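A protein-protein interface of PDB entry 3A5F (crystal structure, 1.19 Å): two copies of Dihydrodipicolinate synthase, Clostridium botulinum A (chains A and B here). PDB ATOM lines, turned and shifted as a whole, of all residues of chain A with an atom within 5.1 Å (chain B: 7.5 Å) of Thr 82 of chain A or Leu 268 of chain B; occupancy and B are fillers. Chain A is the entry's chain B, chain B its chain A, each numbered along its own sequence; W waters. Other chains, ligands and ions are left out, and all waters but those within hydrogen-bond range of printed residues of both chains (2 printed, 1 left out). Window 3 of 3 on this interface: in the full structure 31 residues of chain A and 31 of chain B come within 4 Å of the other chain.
The backbone carbonyl oxygen (O) of Thr 49 of chain B lies within hydrogen-bond range of the side-chain amide nitrogen (ND2) of Asn 81 of chain A.
The side-chain hydroxyl (OG1) of Thr 82 of chain A lies close to the backbone carbonyl oxygen (O) of Leu 268 of chain B, 3.4 Å away.
OG1 of Thr 82 of chain A lies close to N of Pro 269 of chain B, 3.1 Å away.
The side-chain amide oxygen (OD1) of Asn 81 of chain A lies within hydrogen-bond range of the backbone NH (N) of Ala 83 of chain A, 3.0 Å away.
OD1 of Asn 81 of chain A is in hydrogen-bond range of N of Ala 84 of chain A.
The backbone carbonyl oxygen of Asn 81 of chain A is in hydrogen-bond range of the side-chain hydroxyl of Ser 85 of chain A, 2.9 Å away.
OG1 of Thr 82 of chain A sits at hydrogen-bond distance from ND1 of His 118 of chain A, at 2.8 Å.
The backbone carbonyl oxygen (O) of Glu 47 of chain B is in hydrogen-bond range of the side-chain hydroxyl (OG1) of Thr 50 of chain B.
The guanidinium group (NH1) of Arg 267 of chain B sits at hydrogen-bond distance from the backbone carbonyl oxygen (O) of Thr 50 of chain B, 3.0 Å away.
Asn 80 of chain A touches Thr 49 of chain B (OD1 to CG2, 3.2 Å).
CD of Pro 269 of chain B touches O of Asn 80 of chain A (3.2 Å).
Thr 50 of chain B touches Asn 81 of chain A (CA to ND2, 3.7 Å).
CD2 of Leu 268 of chain B touches CB of Lys 117 of chain A, 3.9 Å away.
Cys 271 of chain B touches Lys 117 of chain A.
His 118 of chain A touches Pro 269 of chain B.
Leu 268 of chain B touches just these residues of chain A: Thr 82 (3.1 Å) and Lys 117 (3.9 Å).
Printed residues of chain A within 4 Å of Thr 49 of chain B: Asn 80 (3.2 Å) and Asn 81 (3.3 Å).
Of the printed residues of chain A, Pro 269 of chain B touches Asn 80 (3.2 Å), Thr 82 (3.1 Å) and His 118 (3.9 Å).
Of the printed residues of chain B, Asn 81 of chain A touches Thr 49 and Thr 50.
The nearest residue of chain B that does not touch Thr 82 of chain A is Thr 50 of chain B (5.0 Å).
The nearest residue of chain A that does not touch Leu 268 of chain B is Ala 121 of chain A (4.5 Å).
Hydrophobic or aromatic side chains of chain B within 4 Å of the printed part of chain A: Leu 268 and Pro 269.
Along chain B the printed residues that touch a printed residue of chain A span positions 49 to 271.
Hydrophobic or aromatic side chains of chain A within 4 Å of the printed part of chain B: His 118.
Among the printed residues, no Asp or Glu carboxylate lies within 4 Å of a Lys or Arg side-chain nitrogen of the other chain.
No position is printed for both chains.
Water W2 lies within hydrogen-bond range of O of Leu 268 of chain B (2.8 Å), N of Ala 83 of chain A (3.0 Å) and OD1 of Asn 81 of chain A (3.3 Å).
Water W1 lies within hydrogen-bond range of the side-chain amide nitrogen (ND2) of Asn 81 of chain A (3.1 Å) and the backbone carbonyl oxygen (O) of Thr 49 of chain B (3.4 Å).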
ATOM      1  N   ASN A  80       7.451 -22.169 -19.033  1.00  0.00           N
ATOM      2  CA  ASN A  80       6.409 -22.974 -19.581  1.00  0.00           C
ATOM      3  C   ASN A  80       6.513 -24.439 -19.251  1.00  0.00           C
ATOM      4  O   ASN A  80       5.675 -25.234 -19.655  1.00  0.00           O
ATOM      5  CB  ASN A  80       6.270 -22.690 -21.089  1.00  0.00           C
ATOM      6  CG  ASN A  80       7.501 -22.991 -21.852  1.00  0.00           C
ATOM      7  OD1 ASN A  80       8.528 -23.319 -21.280  1.00  0.00           O
ATOM      8  ND2 ASN A  80       7.396 -22.935 -23.189  1.00  0.00           N
ATOM      9  N   ASN A  81       7.482 -24.767 -18.414  1.00  0.00           N
ATOM     10  CA  ASN A  81       7.668 -26.106 -17.916  1.00  0.00           C
ATOM     11  C   ASN A  81       7.421 -26.042 -16.432  1.00  0.00           C
ATOM     12  O   ASN A  81       8.141 -25.320 -15.693  1.00  0.00           O
ATOM     13  CB  ASN A  81       9.114 -26.529 -18.268  1.00  0.00           C
ATOM     14  CG  ASN A  81       9.575 -27.802 -17.675  1.00  0.00           C
ATOM     15  OD1 ASN A  81       9.132 -28.165 -16.572  1.00  0.00           O
ATOM     16  ND2 ASN A  81      10.549 -28.469 -18.288  1.00  0.00           N
ATOM     17  N   THR A  82       6.423 -26.741 -15.876  1.00  0.00           N
ATOM     18  CA  THR A  82       6.054 -26.607 -14.495  1.00  0.00           C
ATOM     19  C   THR A  82       7.176 -27.069 -13.586  1.00  0.00           C
ATOM     20  O   THR A  82       7.482 -26.411 -12.583  1.00  0.00           O
ATOM     21  CB  THR A  82       4.761 -27.380 -14.215  1.00  0.00           C
ATOM     22  OG1 THR A  82       3.758 -26.981 -15.144  1.00  0.00           O
ATOM     23  CG2 THR A  82       4.263 -27.223 -12.813  1.00  0.00           C
ATOM     24  N   ALA A  83       7.802 -28.221 -13.876  1.00  0.00           N
ATOM     25  CA  ALA A  83       8.886 -28.695 -13.018  1.00  0.00           C
ATOM     26  C   ALA A  83       9.959 -27.665 -12.943  1.00  0.00           C
ATOM     27  O   ALA A  83      10.546 -27.418 -11.861  1.00  0.00           O
ATOM     28  CB  ALA A  83       9.381 -30.040 -13.560  1.00  0.00           C
ATOM     29  N   ALA A  84      10.346 -27.048 -14.064  1.00  0.00           N
ATOM     30  CA  ALA A  84      11.368 -26.066 -14.082  1.00  0.00           C
ATOM     31  C   ALA A  84      11.007 -24.807 -13.273  1.00  0.00           C
ATOM     32  O   ALA A  84      11.837 -24.186 -12.581  1.00  0.00           O
ATOM     33  CB  ALA A  84      11.773 -25.648 -15.528  1.00  0.00           C
ATOM     34  N   SER A  85       9.748 -24.445 -13.346  1.00  0.00           N
ATOM     35  CA  SER A  85       9.244 -23.272 -12.605  1.00  0.00           C
ATOM     36  C   SER A  85       9.302 -23.581 -11.094  1.00  0.00           C
ATOM     37  O   SER A  85       9.665 -22.673 -10.343  1.00  0.00           O
ATOM     38  CB  SER A  85       7.787 -23.061 -13.029  1.00  0.00           C
ATOM     39  OG  SER A  85       7.673 -22.762 -14.393  1.00  0.00           O
ATOM     40  N   ILE A  86       8.932 -24.782 -10.691  1.00  0.00           N
ATOM     41  CA  ILE A  86       9.041 -25.134  -9.292  1.00  0.00           C
ATOM     42  C   ILE A  86      10.491 -25.013  -8.854  1.00  0.00           C
ATOM     43  O   ILE A  86      10.793 -24.452  -7.813  1.00  0.00           O
ATOM     44  CB  ILE A  86       8.489 -26.526  -9.119  1.00  0.00           C
ATOM     45  CG1 ILE A  86       6.986 -26.552  -9.259  1.00  0.00           C
ATOM     46  CG2 ILE A  86       8.978 -27.115  -7.715  1.00  0.00           C
ATOM     47  CD1 ILE A  86       6.384 -27.966  -9.350  1.00  0.00           C
ATOM     48  N   ALA A  87      11.409 -25.608  -9.616  1.00  0.00           N
ATOM     49  CA  ALA A  87      12.817 -25.659  -9.174  1.00  0.00           C
ATOM     50  C   ALA A  87      13.356 -24.233  -9.073  1.00  0.00           C
ATOM     51  O   ALA A  87      14.058 -23.900  -8.126  1.00  0.00           O
ATOM     52  CB  ALA A  87      13.604 -26.503 -10.145  1.00  0.00           C
ATOM     53  N   LYS A 117      -3.692 -26.030 -12.137  1.00  0.00           N
ATOM     54  CA  LYS A 117      -2.696 -27.019 -11.700  1.00  0.00           C
ATOM     55  C   LYS A 117      -1.303 -26.496 -11.698  1.00  0.00           C
ATOM     56  O   LYS A 117      -0.556 -26.789 -10.743  1.00  0.00           O
ATOM     57  CB  LYS A 117      -2.801 -28.258 -12.576  1.00  0.00           C
ATOM     58  CG  LYS A 117      -4.062 -29.056 -12.314  1.00  0.00           C
ATOM     59  CD  LYS A 117      -4.252 -30.163 -13.254  1.00  0.00           C
ATOM     60  CE  LYS A 117      -5.496 -30.967 -13.077  1.00  0.00           C
ATOM     61  NZ  LYS A 117      -5.607 -31.664 -11.878  1.00  0.00           N
ATOM     62  N   HIS A 118      -0.931 -25.731 -12.716  1.00  0.00           N
ATOM     63  CA  HIS A 118       0.403 -25.175 -12.796  1.00  0.00           C
ATOM     64  C   HIS A 118       0.713 -24.254 -11.642  1.00  0.00           C
ATOM     65  O   HIS A 118       1.697 -24.394 -10.938  1.00  0.00           O
ATOM     66  CB  HIS A 118       0.564 -24.431 -14.099  1.00  0.00           C
ATOM     67  CG  HIS A 118       1.838 -23.717 -14.302  1.00  0.00           C
ATOM     68  ND1 HIS A 118       2.979 -24.366 -14.722  1.00  0.00           N
ATOM     69  CD2 HIS A 118       2.134 -22.406 -14.117  1.00  0.00           C
ATOM     70  CE1 HIS A 118       3.939 -23.422 -14.818  1.00  0.00           C
ATOM     71  NE2 HIS A 118       3.470 -22.269 -14.412  1.00  0.00           N
ATOM     72  N   ALA A 121       0.812 -26.009  -8.320  1.00  0.00           N
ATOM     73  CA  ALA A 121       2.015 -26.810  -8.171  1.00  0.00           C
ATOM     74  C   ALA A 121       3.184 -25.928  -7.751  1.00  0.00           C
ATOM     75  O   ALA A 121       4.027 -26.279  -6.909  1.00  0.00           O
ATOM     76  CB  ALA A 121       2.335 -27.651  -9.420  1.00  0.00           C
ATOM     77  N   VAL A 122       3.321 -24.749  -8.376  1.00  0.00           N
ATOM     78  CA  VAL A 122       4.383 -23.816  -7.993  1.00  0.00           C
ATOM     79  C   VAL A 122       4.164 -23.298  -6.591  1.00  0.00           C
ATOM     80  O   VAL A 122       5.066 -23.340  -5.765  1.00  0.00           O
ATOM     81  CB  VAL A 122       4.498 -22.667  -9.045  1.00  0.00           C
ATOM     82  CG1 VAL A 122       5.489 -21.614  -8.508  1.00  0.00           C
ATOM     83  CG2 VAL A 122       4.848 -23.203 -10.434  1.00  0.00           C
ATOM     84  N   GLU B  47       5.718 -32.513 -26.920  1.00  0.00           N
ATOM     85  CA  GLU B  47       5.980 -32.028 -25.570  1.00  0.00           C
ATOM     86  C   GLU B  47       7.423 -31.779 -25.326  1.00  0.00           C
ATOM     87  O   GLU B  47       7.911 -31.911 -24.197  1.00  0.00           O
ATOM     88  CB  GLU B  47       5.343 -32.939 -24.533  1.00  0.00           C
ATOM     89  CG  GLU B  47       3.834 -32.894 -24.485  1.00  0.00           C
ATOM     90  CD  GLU B  47       3.228 -33.884 -23.502  1.00  0.00           C
ATOM     91  OE1 GLU B  47       2.897 -35.023 -23.977  1.00  0.00           O
ATOM     92  OE2 GLU B  47       3.145 -33.628 -22.266  1.00  0.00           O
ATOM     93  N   THR B  49       8.810 -29.022 -24.764  1.00  0.00           N
ATOM     94  CA  THR B  49       8.897 -28.018 -23.675  1.00  0.00           C
ATOM     95  C   THR B  49       9.130 -28.617 -22.345  1.00  0.00           C
ATOM     96  O   THR B  49       9.847 -28.048 -21.503  1.00  0.00           O
ATOM     97  CB  THR B  49       7.599 -27.182 -23.577  1.00  0.00           C
ATOM     98  OG1 THR B  49       7.425 -26.444 -24.788  1.00  0.00           O
ATOM     99  CG2 THR B  49       7.677 -26.222 -22.407  1.00  0.00           C
ATOM    100  N   THR B  50       8.519 -29.729 -22.051  1.00  0.00           N
ATOM    101  CA  THR B  50       8.556 -30.297 -20.741  1.00  0.00           C
ATOM    102  C   THR B  50       9.505 -31.452 -20.624  1.00  0.00           C
ATOM    103  O   THR B  50       9.537 -32.127 -19.630  1.00  0.00           O
ATOM    104  CB  THR B  50       7.178 -30.672 -20.267  1.00  0.00           C
ATOM    105  OG1 THR B  50       6.618 -31.574 -21.207  1.00  0.00           O
ATOM    106  CG2 THR B  50       6.296 -29.432 -20.056  1.00  0.00           C
ATOM    107  N   ASP B 265       0.912 -40.451 -19.634  1.00  0.00           N
ATOM    108  CA  ASP B 265       0.292 -39.212 -19.223  1.00  0.00           C
ATOM    109  C   ASP B 265       1.041 -37.997 -19.753  1.00  0.00           C
ATOM    110  O   ASP B 265       2.159 -38.054 -20.145  1.00  0.00           O
ATOM    111  CB  ASP B 265       0.288 -39.154 -17.713  1.00  0.00           C
ATOM    112  CG  ASP B 265      -0.575 -40.160 -17.099  1.00  0.00           C
ATOM    113  OD1 ASP B 265      -1.541 -40.624 -17.754  1.00  0.00           O
ATOM    114  OD2 ASP B 265      -0.257 -40.506 -15.944  1.00  0.00           O
ATOM    115  N   LEU B 266       0.324 -36.903 -19.803  1.00  0.00           N
ATOM    116  CA  LEU B 266       0.853 -35.601 -20.132  1.00  0.00           C
ATOM    117  C   LEU B 266       1.700 -35.014 -19.032  1.00  0.00           C
ATOM    118  O   LEU B 266       1.397 -35.275 -17.854  1.00  0.00           O
ATOM    119  CB  LEU B 266      -0.317 -34.646 -20.418  1.00  0.00           C
ATOM    120  CG  LEU B 266      -1.168 -34.991 -21.628  1.00  0.00           C
ATOM    121  CD1 LEU B 266      -2.655 -34.660 -21.322  1.00  0.00           C
ATOM    122  CD2 LEU B 266      -0.638 -34.397 -22.864  1.00  0.00           C
ATOM    123  N   ARG B 267       2.658 -34.183 -19.346  1.00  0.00           N
ATOM    124  CA  ARG B 267       3.465 -33.485 -18.323  1.00  0.00           C
ATOM    125  C   ARG B 267       2.889 -32.071 -18.095  1.00  0.00           C
ATOM    126  O   ARG B 267       2.558 -31.339 -19.037  1.00  0.00           O
ATOM    127  CB  ARG B 267       4.934 -33.400 -18.720  1.00  0.00           C
ATOM    128  CG  ARG B 267       5.631 -34.753 -18.652  1.00  0.00           C
ATOM    129  CD  ARG B 267       7.043 -34.674 -19.084  1.00  0.00           C
ATOM    130  NE  ARG B 267       7.746 -35.922 -18.889  1.00  0.00           N
ATOM    131  CZ  ARG B 267       9.035 -36.108 -19.065  1.00  0.00           C
ATOM    132  NH1 ARG B 267       9.771 -35.081 -19.400  1.00  0.00           N
ATOM    133  NH2 ARG B 267       9.615 -37.287 -18.917  1.00  0.00           N
ATOM    134  N   LEU B 268       2.846 -31.670 -16.840  1.00  0.00           N
ATOM    135  CA  LEU B 268       2.387 -30.326 -16.506  1.00  0.00           C
ATOM    136  C   LEU B 268       3.290 -29.275 -17.229  1.00  0.00           C
ATOM    137  O   LEU B 268       4.494 -29.422 -17.337  1.00  0.00           O
ATOM    138  CB  LEU B 268       2.522 -30.098 -15.006  1.00  0.00           C
ATOM    139  CG  LEU B 268       1.418 -30.729 -14.206  1.00  0.00           C
ATOM    140  CD1 LEU B 268       1.771 -30.690 -12.708  1.00  0.00           C
ATOM    141  CD2 LEU B 268       0.045 -30.146 -14.481  1.00  0.00           C
ATOM    142  N   PRO B 269       2.667 -28.219 -17.802  1.00  0.00           N
ATOM    143  CA  PRO B 269       1.354 -27.715 -17.392  1.00  0.00           C
ATOM    144  C   PRO B 269       0.159 -28.297 -18.139  1.00  0.00           C
ATOM    145  O   PRO B 269      -0.938 -27.907 -17.856  1.00  0.00           O
ATOM    146  CB  PRO B 269       1.506 -26.234 -17.752  1.00  0.00           C
ATOM    147  CG  PRO B 269       2.437 -26.236 -18.922  1.00  0.00           C
ATOM    148  CD  PRO B 269       3.470 -27.257 -18.531  1.00  0.00           C
ATOM    149  N   LEU B 270       0.390 -29.257 -19.033  1.00  0.00           N
ATOM    150  CA  LEU B 270      -0.689 -29.980 -19.665  1.00  0.00           C
ATOM    151  C   LEU B 270      -1.289 -30.944 -18.665  1.00  0.00           C
ATOM    152  O   LEU B 270      -0.623 -31.361 -17.751  1.00  0.00           O
ATOM    153  CB  LEU B 270      -0.225 -30.698 -20.928  1.00  0.00           C
ATOM    154  CG  LEU B 270       0.446 -29.826 -21.993  1.00  0.00           C
ATOM    155  CD1 LEU B 270       0.865 -30.722 -23.150  1.00  0.00           C
ATOM    156  CD2 LEU B 270      -0.378 -28.652 -22.410  1.00  0.00           C
ATOM    157  N   CYS B 271      -2.577 -31.258 -18.847  1.00  0.00           N
ATOM    158  CA  CYS B 271      -3.294 -32.090 -17.915  1.00  0.00           C
ATOM    159  C   CYS B 271      -4.466 -32.717 -18.601  1.00  0.00           C
ATOM    160  O   CYS B 271      -4.771 -32.427 -19.755  1.00  0.00           O
ATOM    161  CB  CYS B 271      -3.711 -31.304 -16.691  1.00  0.00           C
ATOM    162  SG  CYS B 271      -4.971 -30.042 -17.043  1.00  0.00           S
ATOM    163  N   GLU B 272      -5.205 -33.503 -17.874  1.00  0.00           N
ATOM    164  CA  GLU B 272      -6.374 -34.202 -18.287  1.00  0.00           C
ATOM    165  C   GLU B 272      -7.446 -33.259 -18.795  1.00  0.00           C
ATOM    166  O   GLU B 272      -7.642 -32.146 -18.247  1.00  0.00           O
ATOM    167  CB  GLU B 272      -6.930 -34.985 -17.084  1.00  0.00           C
ATOM    168  CG  GLU B 272      -6.160 -36.283 -16.896  1.00  0.00           C
ATOM    169  CD  GLU B 272      -6.781 -37.160 -15.857  1.00  0.00           C
ATOM    170  OE1 GLU B 272      -7.842 -36.719 -15.303  1.00  0.00           O
ATOM    171  OE2 GLU B 272      -6.232 -38.250 -15.586  1.00  0.00           O
HETATM  172  O   HOH W   1      12.955 -28.433 -20.191  1.00  0.00           O
HETATM  173  O   HOH W   2       6.660 -30.259 -15.822  1.00  0.00           O
